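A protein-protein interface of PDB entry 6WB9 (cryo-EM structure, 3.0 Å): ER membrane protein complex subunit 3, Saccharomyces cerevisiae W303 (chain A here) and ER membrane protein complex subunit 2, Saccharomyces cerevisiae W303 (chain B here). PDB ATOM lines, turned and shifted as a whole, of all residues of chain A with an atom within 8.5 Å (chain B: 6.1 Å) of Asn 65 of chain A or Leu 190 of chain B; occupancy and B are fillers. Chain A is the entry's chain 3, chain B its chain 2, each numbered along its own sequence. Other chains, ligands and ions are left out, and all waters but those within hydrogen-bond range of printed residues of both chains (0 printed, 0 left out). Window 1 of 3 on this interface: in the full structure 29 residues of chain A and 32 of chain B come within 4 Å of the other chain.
NZ of Lys 74 of chain A lies within hydrogen-bond range of OE1 of Gln 188 of chain B (2.9 Å).
O of Leu 190 of chain B sits at hydrogen-bond distance from ND2 of Asn 65 of chain A.
O of Cys 191 of chain B lies within hydrogen-bond range of ND2 of Asn 62 of chain A, 2.9 Å away.
The side-chain sulfur (SG) of Cys 191 of chain B sits at hydrogen-bond distance from the backbone carbonyl oxygen (O) of Glu 187 of chain B, 3.3 Å away.
The backbone carbonyl oxygen of Asn 62 of chain A is in hydrogen-bond range of the side-chain amide nitrogen of Asn 65 of chain A (3.4 Å).
The backbone carbonyl oxygen of Gly 64 of chain A is in hydrogen-bond range of the backbone NH of Cys 240 of chain A, 2.6 Å away.
The side-chain hydroxyl (OG1) of Thr 239 of chain A sits close to the backbone NH (N) of Leu 241 of chain A, at 3.4 Å.
Leu 58 of chain A touches Cys 191 of chain B (CB to O, 3.9 Å).
Cys 191 of chain B touches Leu 59 of chain A (SG to CD1, 3.8 Å).
Asn 62 of chain A touches Pro 194 of chain B.
CB of Pro 194 of chain B touches ND2 of Asn 65 of chain A, 3.4 Å away.
O of Asn 65 of chain A touches CE1 of Phe 200 of chain B (3.5 Å).
Leu 66 of chain A touches Cys 191 of chain B.
Glu 187 of chain B touches Lys 74 of chain A.
Cys 191 of chain B touches Lys 74 of chain A.
CB of Cys 240 of chain A touches NH1 of Arg 232 of chain B (3.4 Å).
Asn 229 of chain B touches Leu 241 of chain A.
Of chain B, only Leu 190 (3.1 Å), Pro 194 (3.4 Å), Phe 200 (3.5 Å) and Arg 232 (3.6 Å) come within 4 Å of Asn 65 of chain A.
Of chain A, only Leu 58 (3.9 Å), Leu 59 (3.8 Å), Asn 62 (2.9 Å), Leu 66 (3.6 Å) and Lys 74 (3.9 Å) come within 4 Å of Cys 191 of chain B.
Printed residues of chain B within 4 Å of Ala 70 of chain A: Glu 187 (3.4 Å).
Of the printed residues of chain A, Phe 200 of chain B touches Asn 65 (3.5 Å).
Printed residues of chain A within 4 Å of Arg 232 of chain B: Asn 65, Cys 240 and Leu 241.
Of the printed residues of chain B, Asn 62 of chain A touches Cys 191 and Pro 194.
Asp 242 of chain A touches none of the printed residues of chain B.
The nearest residue of chain B that does not touch Asn 65 of chain A is Asn 229 of chain B (4.5 Å).
The nearest printed residue of chain A that does not touch Phe 200 of chain B is Leu 241 of chain A (4.5 Å).
Of the 20 printed residues of chain A, 9 touch a printed residue of chain B.
Hydrophobic or aromatic side chains of chain B that line the printed part of chain A: Pro 194 and Phe 200.
Among the printed residues, 17 pairs touch across the chains.
Among the printed residues, no Asp or Glu carboxylate lies within 4 Å of a Lys or Arg side-chain nitrogen of the other chain.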
ATOM      1  N   LEU A  58      31.824  17.271 -15.720  1.00  0.00           N
ATOM      2  CA  LEU A  58      30.513  17.569 -16.282  1.00  0.00           C
ATOM      3  C   LEU A  58      30.622  18.226 -17.646  1.00  0.00           C
ATOM      4  O   LEU A  58      29.735  18.046 -18.479  1.00  0.00           O
ATOM      5  CB  LEU A  58      29.714  18.465 -15.338  1.00  0.00           C
ATOM      6  CG  LEU A  58      29.034  17.791 -14.148  1.00  0.00           C
ATOM      7  CD1 LEU A  58      28.215  18.803 -13.376  1.00  0.00           C
ATOM      8  CD2 LEU A  58      28.166  16.637 -14.608  1.00  0.00           C
ATOM      9  N   LEU A  59      31.694  18.981 -17.894  1.00  0.00           N
ATOM     10  CA  LEU A  59      31.928  19.515 -19.232  1.00  0.00           C
ATOM     11  C   LEU A  59      32.228  18.394 -20.219  1.00  0.00           C
ATOM     12  O   LEU A  59      31.704  18.400 -21.339  1.00  0.00           O
ATOM     13  CB  LEU A  59      33.069  20.527 -19.197  1.00  0.00           C
ATOM     14  CG  LEU A  59      33.311  21.333 -20.472  1.00  0.00           C
ATOM     15  CD1 LEU A  59      32.099  22.179 -20.808  1.00  0.00           C
ATOM     16  CD2 LEU A  59      34.541  22.204 -20.318  1.00  0.00           C
ATOM     17  N   ILE A  60      33.025  17.405 -19.791  1.00  0.00           N
ATOM     18  CA  ILE A  60      33.275  16.204 -20.592  1.00  0.00           C
ATOM     19  C   ILE A  60      31.971  15.465 -20.882  1.00  0.00           C
ATOM     20  O   ILE A  60      31.689  15.088 -22.027  1.00  0.00           O
ATOM     21  CB  ILE A  60      34.290  15.294 -19.872  1.00  0.00           C
ATOM     22  CG1 ILE A  60      35.699  15.872 -19.980  1.00  0.00           C
ATOM     23  CG2 ILE A  60      34.258  13.868 -20.421  1.00  0.00           C
ATOM     24  CD1 ILE A  60      36.220  15.901 -21.387  1.00  0.00           C
ATOM     25  N   GLY A  61      31.137  15.287 -19.857  1.00  0.00           N
ATOM     26  CA  GLY A  61      29.927  14.500 -20.022  1.00  0.00           C
ATOM     27  C   GLY A  61      28.787  15.216 -20.718  1.00  0.00           C
ATOM     28  O   GLY A  61      27.919  14.563 -21.305  1.00  0.00           O
ATOM     29  N   ASN A  62      28.762  16.549 -20.671  1.00  0.00           N
ATOM     30  CA  ASN A  62      27.629  17.321 -21.161  1.00  0.00           C
ATOM     31  C   ASN A  62      28.065  18.426 -22.116  1.00  0.00           C
ATOM     32  O   ASN A  62      27.395  19.455 -22.220  1.00  0.00           O
ATOM     33  CB  ASN A  62      26.838  17.920 -19.997  1.00  0.00           C
ATOM     34  CG  ASN A  62      26.335  16.870 -19.030  1.00  0.00           C
ATOM     35  OD1 ASN A  62      25.962  15.770 -19.429  1.00  0.00           O
ATOM     36  ND2 ASN A  62      26.320  17.208 -17.747  1.00  0.00           N
ATOM     37  N   GLY A  63      29.190  18.241 -22.814  1.00  0.00           N
ATOM     38  CA  GLY A  63      29.522  19.148 -23.897  1.00  0.00           C
ATOM     39  C   GLY A  63      28.611  19.046 -25.101  1.00  0.00           C
ATOM     40  O   GLY A  63      28.593  19.967 -25.924  1.00  0.00           O
ATOM     41  N   GLY A  64      27.852  17.954 -25.222  1.00  0.00           N
ATOM     42  CA  GLY A  64      26.924  17.790 -26.327  1.00  0.00           C
ATOM     43  C   GLY A  64      25.773  18.773 -26.328  1.00  0.00           C
ATOM     44  O   GLY A  64      25.175  19.010 -27.381  1.00  0.00           O
ATOM     45  N   ASN A  65      25.450  19.352 -25.173  1.00  0.00           N
ATOM     46  CA  ASN A  65      24.380  20.335 -25.088  1.00  0.00           C
ATOM     47  C   ASN A  65      24.775  21.686 -25.662  1.00  0.00           C
ATOM     48  O   ASN A  65      23.895  22.454 -26.063  1.00  0.00           O
ATOM     49  CB  ASN A  65      23.951  20.516 -23.634  1.00  0.00           C
ATOM     50  CG  ASN A  65      23.633  19.209 -22.957  1.00  0.00           C
ATOM     51  OD1 ASN A  65      23.008  18.325 -23.543  1.00  0.00           O
ATOM     52  ND2 ASN A  65      24.071  19.072 -21.717  1.00  0.00           N
ATOM     53  N   LEU A  66      26.065  21.997 -25.700  1.00  0.00           N
ATOM     54  CA  LEU A  66      26.528  23.301 -26.139  1.00  0.00           C
ATOM     55  C   LEU A  66      26.823  23.295 -27.634  1.00  0.00           C
ATOM     56  O   LEU A  66      26.784  22.262 -28.304  1.00  0.00           O
ATOM     57  CB  LEU A  66      27.781  23.709 -25.370  1.00  0.00           C
ATOM     58  CG  LEU A  66      27.891  23.265 -23.915  1.00  0.00           C
ATOM     59  CD1 LEU A  66      29.296  23.505 -23.414  1.00  0.00           C
ATOM     60  CD2 LEU A  66      26.892  24.009 -23.067  1.00  0.00           C
ATOM     61  N   SER A  67      27.126  24.477 -28.155  1.00  0.00           N
ATOM     62  CA  SER A  67      27.656  24.613 -29.501  1.00  0.00           C
ATOM     63  C   SER A  67      29.173  24.448 -29.442  1.00  0.00           C
ATOM     64  O   SER A  67      29.737  24.069 -28.412  1.00  0.00           O
ATOM     65  CB  SER A  67      27.239  25.954 -30.100  1.00  0.00           C
ATOM     66  OG  SER A  67      27.704  27.031 -29.308  1.00  0.00           O
ATOM     67  N   SER A  68      29.861  24.731 -30.546  1.00  0.00           N
ATOM     68  CA  SER A  68      31.317  24.657 -30.524  1.00  0.00           C
ATOM     69  C   SER A  68      31.928  25.935 -29.960  1.00  0.00           C
ATOM     70  O   SER A  68      32.927  25.879 -29.232  1.00  0.00           O
ATOM     71  CB  SER A  68      31.850  24.376 -31.928  1.00  0.00           C
ATOM     72  OG  SER A  68      31.383  23.125 -32.403  1.00  0.00           O
ATOM     73  N   ALA A  70      30.966  27.841 -27.620  1.00  0.00           N
ATOM     74  CA  ALA A  70      30.883  27.929 -26.168  1.00  0.00           C
ATOM     75  C   ALA A  70      31.607  26.798 -25.461  1.00  0.00           C
ATOM     76  O   ALA A  70      32.215  27.024 -24.410  1.00  0.00           O
ATOM     77  CB  ALA A  70      29.421  27.941 -25.724  1.00  0.00           C
ATOM     78  N   PHE A  71      31.550  25.584 -26.019  1.00  0.00           N
ATOM     79  CA  PHE A  71      32.309  24.471 -25.461  1.00  0.00           C
ATOM     80  C   PHE A  71      33.807  24.698 -25.588  1.00  0.00           C
ATOM     81  O   PHE A  71      34.560  24.303 -24.695  1.00  0.00           O
ATOM     82  CB  PHE A  71      31.916  23.160 -26.139  1.00  0.00           C
ATOM     83  CG  PHE A  71      32.712  21.974 -25.674  1.00  0.00           C
ATOM     84  CD1 PHE A  71      32.495  21.426 -24.421  1.00  0.00           C
ATOM     85  CD2 PHE A  71      33.675  21.402 -26.492  1.00  0.00           C
ATOM     86  CE1 PHE A  71      33.224  20.334 -23.990  1.00  0.00           C
ATOM     87  CE2 PHE A  71      34.407  20.310 -26.067  1.00  0.00           C
ATOM     88  CZ  PHE A  71      34.180  19.776 -24.813  1.00  0.00           C
ATOM     89  N   LYS A  74      34.636  27.262 -22.759  1.00  0.00           N
ATOM     90  CA  LYS A  74      34.591  26.603 -21.458  1.00  0.00           C
ATOM     91  C   LYS A  74      35.724  25.600 -21.290  1.00  0.00           C
ATOM     92  O   LYS A  74      36.272  25.477 -20.192  1.00  0.00           O
ATOM     93  CB  LYS A  74      33.243  25.914 -21.258  1.00  0.00           C
ATOM     94  CG  LYS A  74      32.102  26.869 -20.988  1.00  0.00           C
ATOM     95  CD  LYS A  74      30.828  26.124 -20.655  1.00  0.00           C
ATOM     96  CE  LYS A  74      29.728  27.093 -20.272  1.00  0.00           C
ATOM     97  NZ  LYS A  74      30.127  27.939 -19.117  1.00  0.00           N
ATOM     98  N   HIS A 237      34.835  16.798 -29.508  1.00  0.00           N
ATOM     99  CA  HIS A 237      33.551  17.458 -29.317  1.00  0.00           C
ATOM    100  C   HIS A 237      32.532  16.918 -30.313  1.00  0.00           C
ATOM    101  O   HIS A 237      32.711  17.045 -31.528  1.00  0.00           O
ATOM    102  CB  HIS A 237      33.707  18.967 -29.475  1.00  0.00           C
ATOM    103  CG  HIS A 237      32.432  19.727 -29.294  1.00  0.00           C
ATOM    104  ND1 HIS A 237      31.585  19.517 -28.227  1.00  0.00           N
ATOM    105  CD2 HIS A 237      31.862  20.703 -30.039  1.00  0.00           C
ATOM    106  CE1 HIS A 237      30.548  20.329 -28.325  1.00  0.00           C
ATOM    107  NE2 HIS A 237      30.691  21.059 -29.415  1.00  0.00           N
ATOM    108  N   GLU A 238      31.464  16.311 -29.796  1.00  0.00           N
ATOM    109  CA  GLU A 238      30.372  15.773 -30.608  1.00  0.00           C
ATOM    110  C   GLU A 238      29.077  16.357 -30.052  1.00  0.00           C
ATOM    111  O   GLU A 238      28.423  15.743 -29.205  1.00  0.00           O
ATOM    112  CB  GLU A 238      30.367  14.247 -30.586  1.00  0.00           C
ATOM    113  CG  GLU A 238      31.611  13.614 -31.188  1.00  0.00           C
ATOM    114  CD  GLU A 238      31.732  12.139 -30.866  1.00  0.00           C
ATOM    115  OE1 GLU A 238      31.004  11.664 -29.969  1.00  0.00           O
ATOM    116  OE2 GLU A 238      32.555  11.454 -31.508  1.00  0.00           O
ATOM    117  N   THR A 239      28.710  17.543 -30.530  1.00  0.00           N
ATOM    118  CA  THR A 239      27.562  18.252 -29.991  1.00  0.00           C
ATOM    119  C   THR A 239      26.257  17.664 -30.512  1.00  0.00           C
ATOM    120  O   THR A 239      26.191  17.112 -31.614  1.00  0.00           O
ATOM    121  CB  THR A 239      27.633  19.740 -30.337  1.00  0.00           C
ATOM    122  OG1 THR A 239      26.613  20.449 -29.625  1.00  0.00           O
ATOM    123  CG2 THR A 239      27.452  19.956 -31.825  1.00  0.00           C
ATOM    124  N   CYS A 240      25.212  17.784 -29.698  1.00  0.00           N
ATOM    125  CA  CYS A 240      23.884  17.309 -30.055  1.00  0.00           C
ATOM    126  C   CYS A 240      23.038  18.384 -30.723  1.00  0.00           C
ATOM    127  O   CYS A 240      21.838  18.174 -30.923  1.00  0.00           O
ATOM    128  CB  CYS A 240      23.160  16.780 -28.814  1.00  0.00           C
ATOM    129  SG  CYS A 240      24.043  15.482 -27.918  1.00  0.00           S
ATOM    130  N   LEU A 241      23.632  19.523 -31.069  1.00  0.00           N
ATOM    131  CA  LEU A 241      22.915  20.617 -31.704  1.00  0.00           C
ATOM    132  C   LEU A 241      23.132  20.680 -33.208  1.00  0.00           C
ATOM    133  O   LEU A 241      22.558  21.555 -33.859  1.00  0.00           O
ATOM    134  CB  LEU A 241      23.327  21.955 -31.081  1.00  0.00           C
ATOM    135  CG  LEU A 241      22.996  22.186 -29.609  1.00  0.00           C
ATOM    136  CD1 LEU A 241      23.391  23.589 -29.196  1.00  0.00           C
ATOM    137  CD2 LEU A 241      21.525  21.959 -29.368  1.00  0.00           C
ATOM    138  N   ASP A 242      23.943  19.783 -33.774  1.00  0.00           N
ATOM    139  CA  ASP A 242      24.252  19.847 -35.200  1.00  0.00           C
ATOM    140  C   ASP A 242      23.044  19.463 -36.048  1.00  0.00           C
ATOM    141  O   ASP A 242      22.581  20.247 -36.884  1.00  0.00           O
ATOM    142  CB  ASP A 242      25.442  18.943 -35.523  1.00  0.00           C
ATOM    143  CG  ASP A 242      26.766  19.564 -35.138  1.00  0.00           C
ATOM    144  OD1 ASP A 242      26.830  20.805 -35.014  1.00  0.00           O
ATOM    145  OD2 ASP A 242      27.748  18.811 -34.968  1.00  0.00           O
ATOM    146  N   CYS B 185      26.189  31.980 -19.052  1.00  0.00           N
ATOM    147  CA  CYS B 185      25.651  31.425 -17.811  1.00  0.00           C
ATOM    148  C   CYS B 185      24.619  30.331 -18.080  1.00  0.00           C
ATOM    149  O   CYS B 185      24.583  29.316 -17.373  1.00  0.00           O
ATOM    150  CB  CYS B 185      25.042  32.537 -16.963  1.00  0.00           C
ATOM    151  SG  CYS B 185      26.222  33.759 -16.360  1.00  0.00           S
ATOM    152  N   LEU B 186      23.791  30.505 -19.114  1.00  0.00           N
ATOM    153  CA  LEU B 186      22.796  29.487 -19.441  1.00  0.00           C
ATOM    154  C   LEU B 186      23.448  28.229 -20.003  1.00  0.00           C
ATOM    155  O   LEU B 186      23.004  27.114 -19.708  1.00  0.00           O
ATOM    156  CB  LEU B 186      21.772  30.047 -20.421  1.00  0.00           C
ATOM    157  CG  LEU B 186      20.837  31.093 -19.818  1.00  0.00           C
ATOM    158  CD1 LEU B 186      20.114  31.837 -20.905  1.00  0.00           C
ATOM    159  CD2 LEU B 186      19.859  30.450 -18.880  1.00  0.00           C
ATOM    160  N   GLU B 187      24.514  28.380 -20.791  1.00  0.00           N
ATOM    161  CA  GLU B 187      25.262  27.211 -21.242  1.00  0.00           C
ATOM    162  C   GLU B 187      25.964  26.517 -20.082  1.00  0.00           C
ATOM    163  O   GLU B 187      26.129  25.291 -20.099  1.00  0.00           O
ATOM    164  CB  GLU B 187      26.259  27.620 -22.324  1.00  0.00           C
ATOM    165  CG  GLU B 187      25.613  27.864 -23.678  1.00  0.00           C
ATOM    166  CD  GLU B 187      26.299  28.959 -24.471  1.00  0.00           C
ATOM    167  OE1 GLU B 187      27.177  29.642 -23.903  1.00  0.00           O
ATOM    168  OE2 GLU B 187      25.965  29.138 -25.660  1.00  0.00           O
ATOM    169  N   GLN B 188      26.333  27.268 -19.043  1.00  0.00           N
ATOM    170  CA  GLN B 188      26.871  26.625 -17.848  1.00  0.00           C
ATOM    171  C   GLN B 188      25.799  25.835 -17.100  1.00  0.00           C
ATOM    172  O   GLN B 188      26.077  24.744 -16.583  1.00  0.00           O
ATOM    173  CB  GLN B 188      27.513  27.664 -16.936  1.00  0.00           C
ATOM    174  CG  GLN B 188      28.232  27.053 -15.761  1.00  0.00           C
ATOM    175  CD  GLN B 188      29.066  25.857 -16.147  1.00  0.00           C
ATOM    176  OE1 GLN B 188      29.971  25.952 -16.975  1.00  0.00           O
ATOM    177  NE2 GLN B 188      28.768  24.716 -15.544  1.00  0.00           N
ATOM    178  N   VAL B 189      24.572  26.369 -17.035  1.00  0.00           N
ATOM    179  CA  VAL B 189      23.461  25.621 -16.433  1.00  0.00           C
ATOM    180  C   VAL B 189      23.173  24.355 -17.238  1.00  0.00           C
ATOM    181  O   VAL B 189      22.869  23.295 -16.674  1.00  0.00           O
ATOM    182  CB  VAL B 189      22.209  26.513 -16.308  1.00  0.00           C
ATOM    183  CG1 VAL B 189      21.042  25.752 -15.709  1.00  0.00           C
ATOM    184  CG2 VAL B 189      22.487  27.702 -15.453  1.00  0.00           C
ATOM    185  N   LEU B 190      23.311  24.436 -18.564  1.00  0.00           N
ATOM    186  CA  LEU B 190      23.183  23.248 -19.409  1.00  0.00           C
ATOM    187  C   LEU B 190      24.299  22.244 -19.163  1.00  0.00           C
ATOM    188  O   LEU B 190      24.087  21.038 -19.320  1.00  0.00           O
ATOM    189  CB  LEU B 190      23.177  23.645 -20.879  1.00  0.00           C
ATOM    190  CG  LEU B 190      21.958  24.428 -21.331  1.00  0.00           C
ATOM    191  CD1 LEU B 190      22.138  24.840 -22.764  1.00  0.00           C
ATOM    192  CD2 LEU B 190      20.727  23.579 -21.158  1.00  0.00           C
ATOM    193  N   CYS B 191      25.496  22.720 -18.814  1.00  0.00           N
ATOM    194  CA  CYS B 191      26.555  21.802 -18.407  1.00  0.00           C
ATOM    195  C   CYS B 191      26.221  21.124 -17.084  1.00  0.00           C
ATOM    196  O   CYS B 191      26.502  19.934 -16.905  1.00  0.00           O
ATOM    197  CB  CYS B 191      27.889  22.537 -18.299  1.00  0.00           C
ATOM    198  SG  CYS B 191      28.575  23.063 -19.868  1.00  0.00           S
ATOM    199  N   ILE B 192      25.619  21.861 -16.149  1.00  0.00           N
ATOM    200  CA  ILE B 192      25.303  21.292 -14.839  1.00  0.00           C
ATOM    201  C   ILE B 192      24.113  20.344 -14.937  1.00  0.00           C
ATOM    202  O   ILE B 192      24.217  19.152 -14.624  1.00  0.00           O
ATOM    203  CB  ILE B 192      25.043  22.408 -13.814  1.00  0.00           C
ATOM    204  CG1 ILE B 192      26.284  23.280 -13.658  1.00  0.00           C
ATOM    205  CG2 ILE B 192      24.653  21.811 -12.477  1.00  0.00           C
ATOM    206  CD1 ILE B 192      25.985  24.680 -13.199  1.00  0.00           C
ATOM    207  N   THR B 193      22.960  20.863 -15.360  1.00  0.00           N
ATOM    208  CA  THR B 193      21.768  20.051 -15.560  1.00  0.00           C
ATOM    209  C   THR B 193      21.570  19.844 -17.053  1.00  0.00           C
ATOM    210  O   THR B 193      21.100  20.761 -17.742  1.00  0.00           O
ATOM    211  CB  THR B 193      20.540  20.722 -14.941  1.00  0.00           C
ATOM    212  OG1 THR B 193      20.421  22.057 -15.441  1.00  0.00           O
ATOM    213  CG2 THR B 193      20.664  20.763 -13.433  1.00  0.00           C
ATOM    214  N   PRO B 194      21.903  18.671 -17.600  1.00  0.00           N
ATOM    215  CA  PRO B 194      21.908  18.519 -19.063  1.00  0.00           C
ATOM    216  C   PRO B 194      20.526  18.448 -19.687  1.00  0.00           C
ATOM    217  O   PRO B 194      20.373  18.822 -20.857  1.00  0.00           O
ATOM    218  CB  PRO B 194      22.681  17.210 -19.268  1.00  0.00           C
ATOM    219  CG  PRO B 194      22.438  16.443 -18.019  1.00  0.00           C
ATOM    220  CD  PRO B 194      22.369  17.454 -16.914  1.00  0.00           C
ATOM    221  N   PHE B 195      19.518  17.985 -18.953  1.00  0.00           N
ATOM    222  CA  PHE B 195      18.181  17.793 -19.493  1.00  0.00           C
ATOM    223  C   PHE B 195      17.242  18.932 -19.128  1.00  0.00           C
ATOM    224  O   PHE B 195      16.021  18.771 -19.194  1.00  0.00           O
ATOM    225  CB  PHE B 195      17.614  16.458 -19.014  1.00  0.00           C
ATOM    226  CG  PHE B 195      18.498  15.287 -19.321  1.00  0.00           C
ATOM    227  CD1 PHE B 195      19.117  15.172 -20.555  1.00  0.00           C
ATOM    228  CD2 PHE B 195      18.723  14.308 -18.369  1.00  0.00           C
ATOM    229  CE1 PHE B 195      19.938  14.101 -20.838  1.00  0.00           C
ATOM    230  CE2 PHE B 195      19.542  13.231 -18.647  1.00  0.00           C
ATOM    231  CZ  PHE B 195      20.149  13.128 -19.883  1.00  0.00           C
ATOM    232  N   ASN B 196      17.793  20.079 -18.747  1.00  0.00           N
ATOM    233  CA  ASN B 196      17.015  21.257 -18.376  1.00  0.00           C
ATOM    234  C   ASN B 196      16.487  21.878 -19.660  1.00  0.00           C
ATOM    235  O   ASN B 196      17.136  22.722 -20.278  1.00  0.00           O
ATOM    236  CB  ASN B 196      17.882  22.231 -17.589  1.00  0.00           C
ATOM    237  CG  ASN B 196      17.075  23.169 -16.723  1.00  0.00           C
ATOM    238  OD1 ASN B 196      15.908  23.437 -16.993  1.00  0.00           O
ATOM    239  ND2 ASN B 196      17.699  23.676 -15.671  1.00  0.00           N
ATOM    240  N   TYR B 197      15.294  21.442 -20.079  1.00  0.00           N
ATOM    241  CA  TYR B 197      14.713  21.960 -21.314  1.00  0.00           C
ATOM    242  C   TYR B 197      14.242  23.398 -21.149  1.00  0.00           C
ATOM    243  O   TYR B 197      14.170  24.142 -22.135  1.00  0.00           O
ATOM    244  CB  TYR B 197      13.567  21.062 -21.785  1.00  0.00           C
ATOM    245  CG  TYR B 197      12.384  20.960 -20.848  1.00  0.00           C
ATOM    246  CD1 TYR B 197      12.352  20.013 -19.832  1.00  0.00           C
ATOM    247  CD2 TYR B 197      11.281  21.792 -20.999  1.00  0.00           C
ATOM    248  CE1 TYR B 197      11.269  19.916 -18.982  1.00  0.00           C
ATOM    249  CE2 TYR B 197      10.200  21.704 -20.155  1.00  0.00           C
ATOM    250  CZ  TYR B 197      10.197  20.764 -19.152  1.00  0.00           C
ATOM    251  OH  TYR B 197       9.110  20.679 -18.318  1.00  0.00           O
ATOM    252  N   CYS B 199      16.051  25.514 -19.570  1.00  0.00           N
ATOM    253  CA  CYS B 199      17.279  26.256 -19.815  1.00  0.00           C
ATOM    254  C   CYS B 199      17.601  26.342 -21.299  1.00  0.00           C
ATOM    255  O   CYS B 199      18.136  27.358 -21.751  1.00  0.00           O
ATOM    256  CB  CYS B 199      18.435  25.618 -19.059  1.00  0.00           C
ATOM    257  SG  CYS B 199      19.908  26.607 -19.124  1.00  0.00           S
ATOM    258  N   PHE B 200      17.280  25.297 -22.071  1.00  0.00           N
ATOM    259  CA  PHE B 200      17.408  25.377 -23.523  1.00  0.00           C
ATOM    260  C   PHE B 200      16.450  26.406 -24.102  1.00  0.00           C
ATOM    261  O   PHE B 200      16.812  27.154 -25.017  1.00  0.00           O
ATOM    262  CB  PHE B 200      17.151  24.012 -24.156  1.00  0.00           C
ATOM    263  CG  PHE B 200      18.349  23.119 -24.193  1.00  0.00           C
ATOM    264  CD1 PHE B 200      19.423  23.420 -25.009  1.00  0.00           C
ATOM    265  CD2 PHE B 200      18.385  21.959 -23.439  1.00  0.00           C
ATOM    266  CE1 PHE B 200      20.519  22.592 -25.057  1.00  0.00           C
ATOM    267  CE2 PHE B 200      19.481  21.127 -23.484  1.00  0.00           C
ATOM    268  CZ  PHE B 200      20.549  21.447 -24.290  1.00  0.00           C
ATOM    269  N   LEU B 203      17.896  29.820 -23.215  1.00  0.00           N
ATOM    270  CA  LEU B 203      19.040  30.111 -24.071  1.00  0.00           C
ATOM    271  C   LEU B 203      18.595  30.480 -25.479  1.00  0.00           C
ATOM    272  O   LEU B 203      19.155  31.399 -26.093  1.00  0.00           O
ATOM    273  CB  LEU B 203      19.984  28.910 -24.102  1.00  0.00           C
ATOM    274  CG  LEU B 203      21.248  29.089 -24.935  1.00  0.00           C
ATOM    275  CD1 LEU B 203      22.042  30.244 -24.400  1.00  0.00           C
ATOM    276  CD2 LEU B 203      22.083  27.839 -24.928  1.00  0.00           C
ATOM    277  N   ASN B 229      18.728  25.630 -30.363  1.00  0.00           N
ATOM    278  CA  ASN B 229      18.457  25.455 -28.939  1.00  0.00           C
ATOM    279  C   ASN B 229      16.966  25.302 -28.657  1.00  0.00           C
ATOM    280  O   ASN B 229      16.588  24.541 -27.760  1.00  0.00           O
ATOM    281  CB  ASN B 229      19.038  26.620 -28.145  1.00  0.00           C
ATOM    282  CG  ASN B 229      20.545  26.585 -28.101  1.00  0.00           C
ATOM    283  OD1 ASN B 229      21.135  25.785 -27.379  1.00  0.00           O
ATOM    284  ND2 ASN B 229      21.179  27.448 -28.880  1.00  0.00           N
ATOM    285  N   ARG B 232      16.260  21.770 -29.493  1.00  0.00           N
ATOM    286  CA  ARG B 232      16.710  20.882 -28.429  1.00  0.00           C
ATOM    287  C   ARG B 232      15.794  20.959 -27.214  1.00  0.00           C
ATOM    288  O   ARG B 232      15.654  19.972 -26.483  1.00  0.00           O
ATOM    289  CB  ARG B 232      18.148  21.211 -28.040  1.00  0.00           C
ATOM    290  CG  ARG B 232      18.807  20.161 -27.164  1.00  0.00           C
ATOM    291  CD  ARG B 232      18.810  18.803 -27.834  1.00  0.00           C
ATOM    292  NE  ARG B 232      18.718  17.709 -26.872  1.00  0.00           N
ATOM    293  CZ  ARG B 232      19.753  17.199 -26.215  1.00  0.00           C
ATOM    294  NH1 ARG B 232      20.969  17.684 -26.406  1.00  0.00           N
ATOM    295  NH2 ARG B 232      19.573  16.203 -25.362  1.00  0.00           N
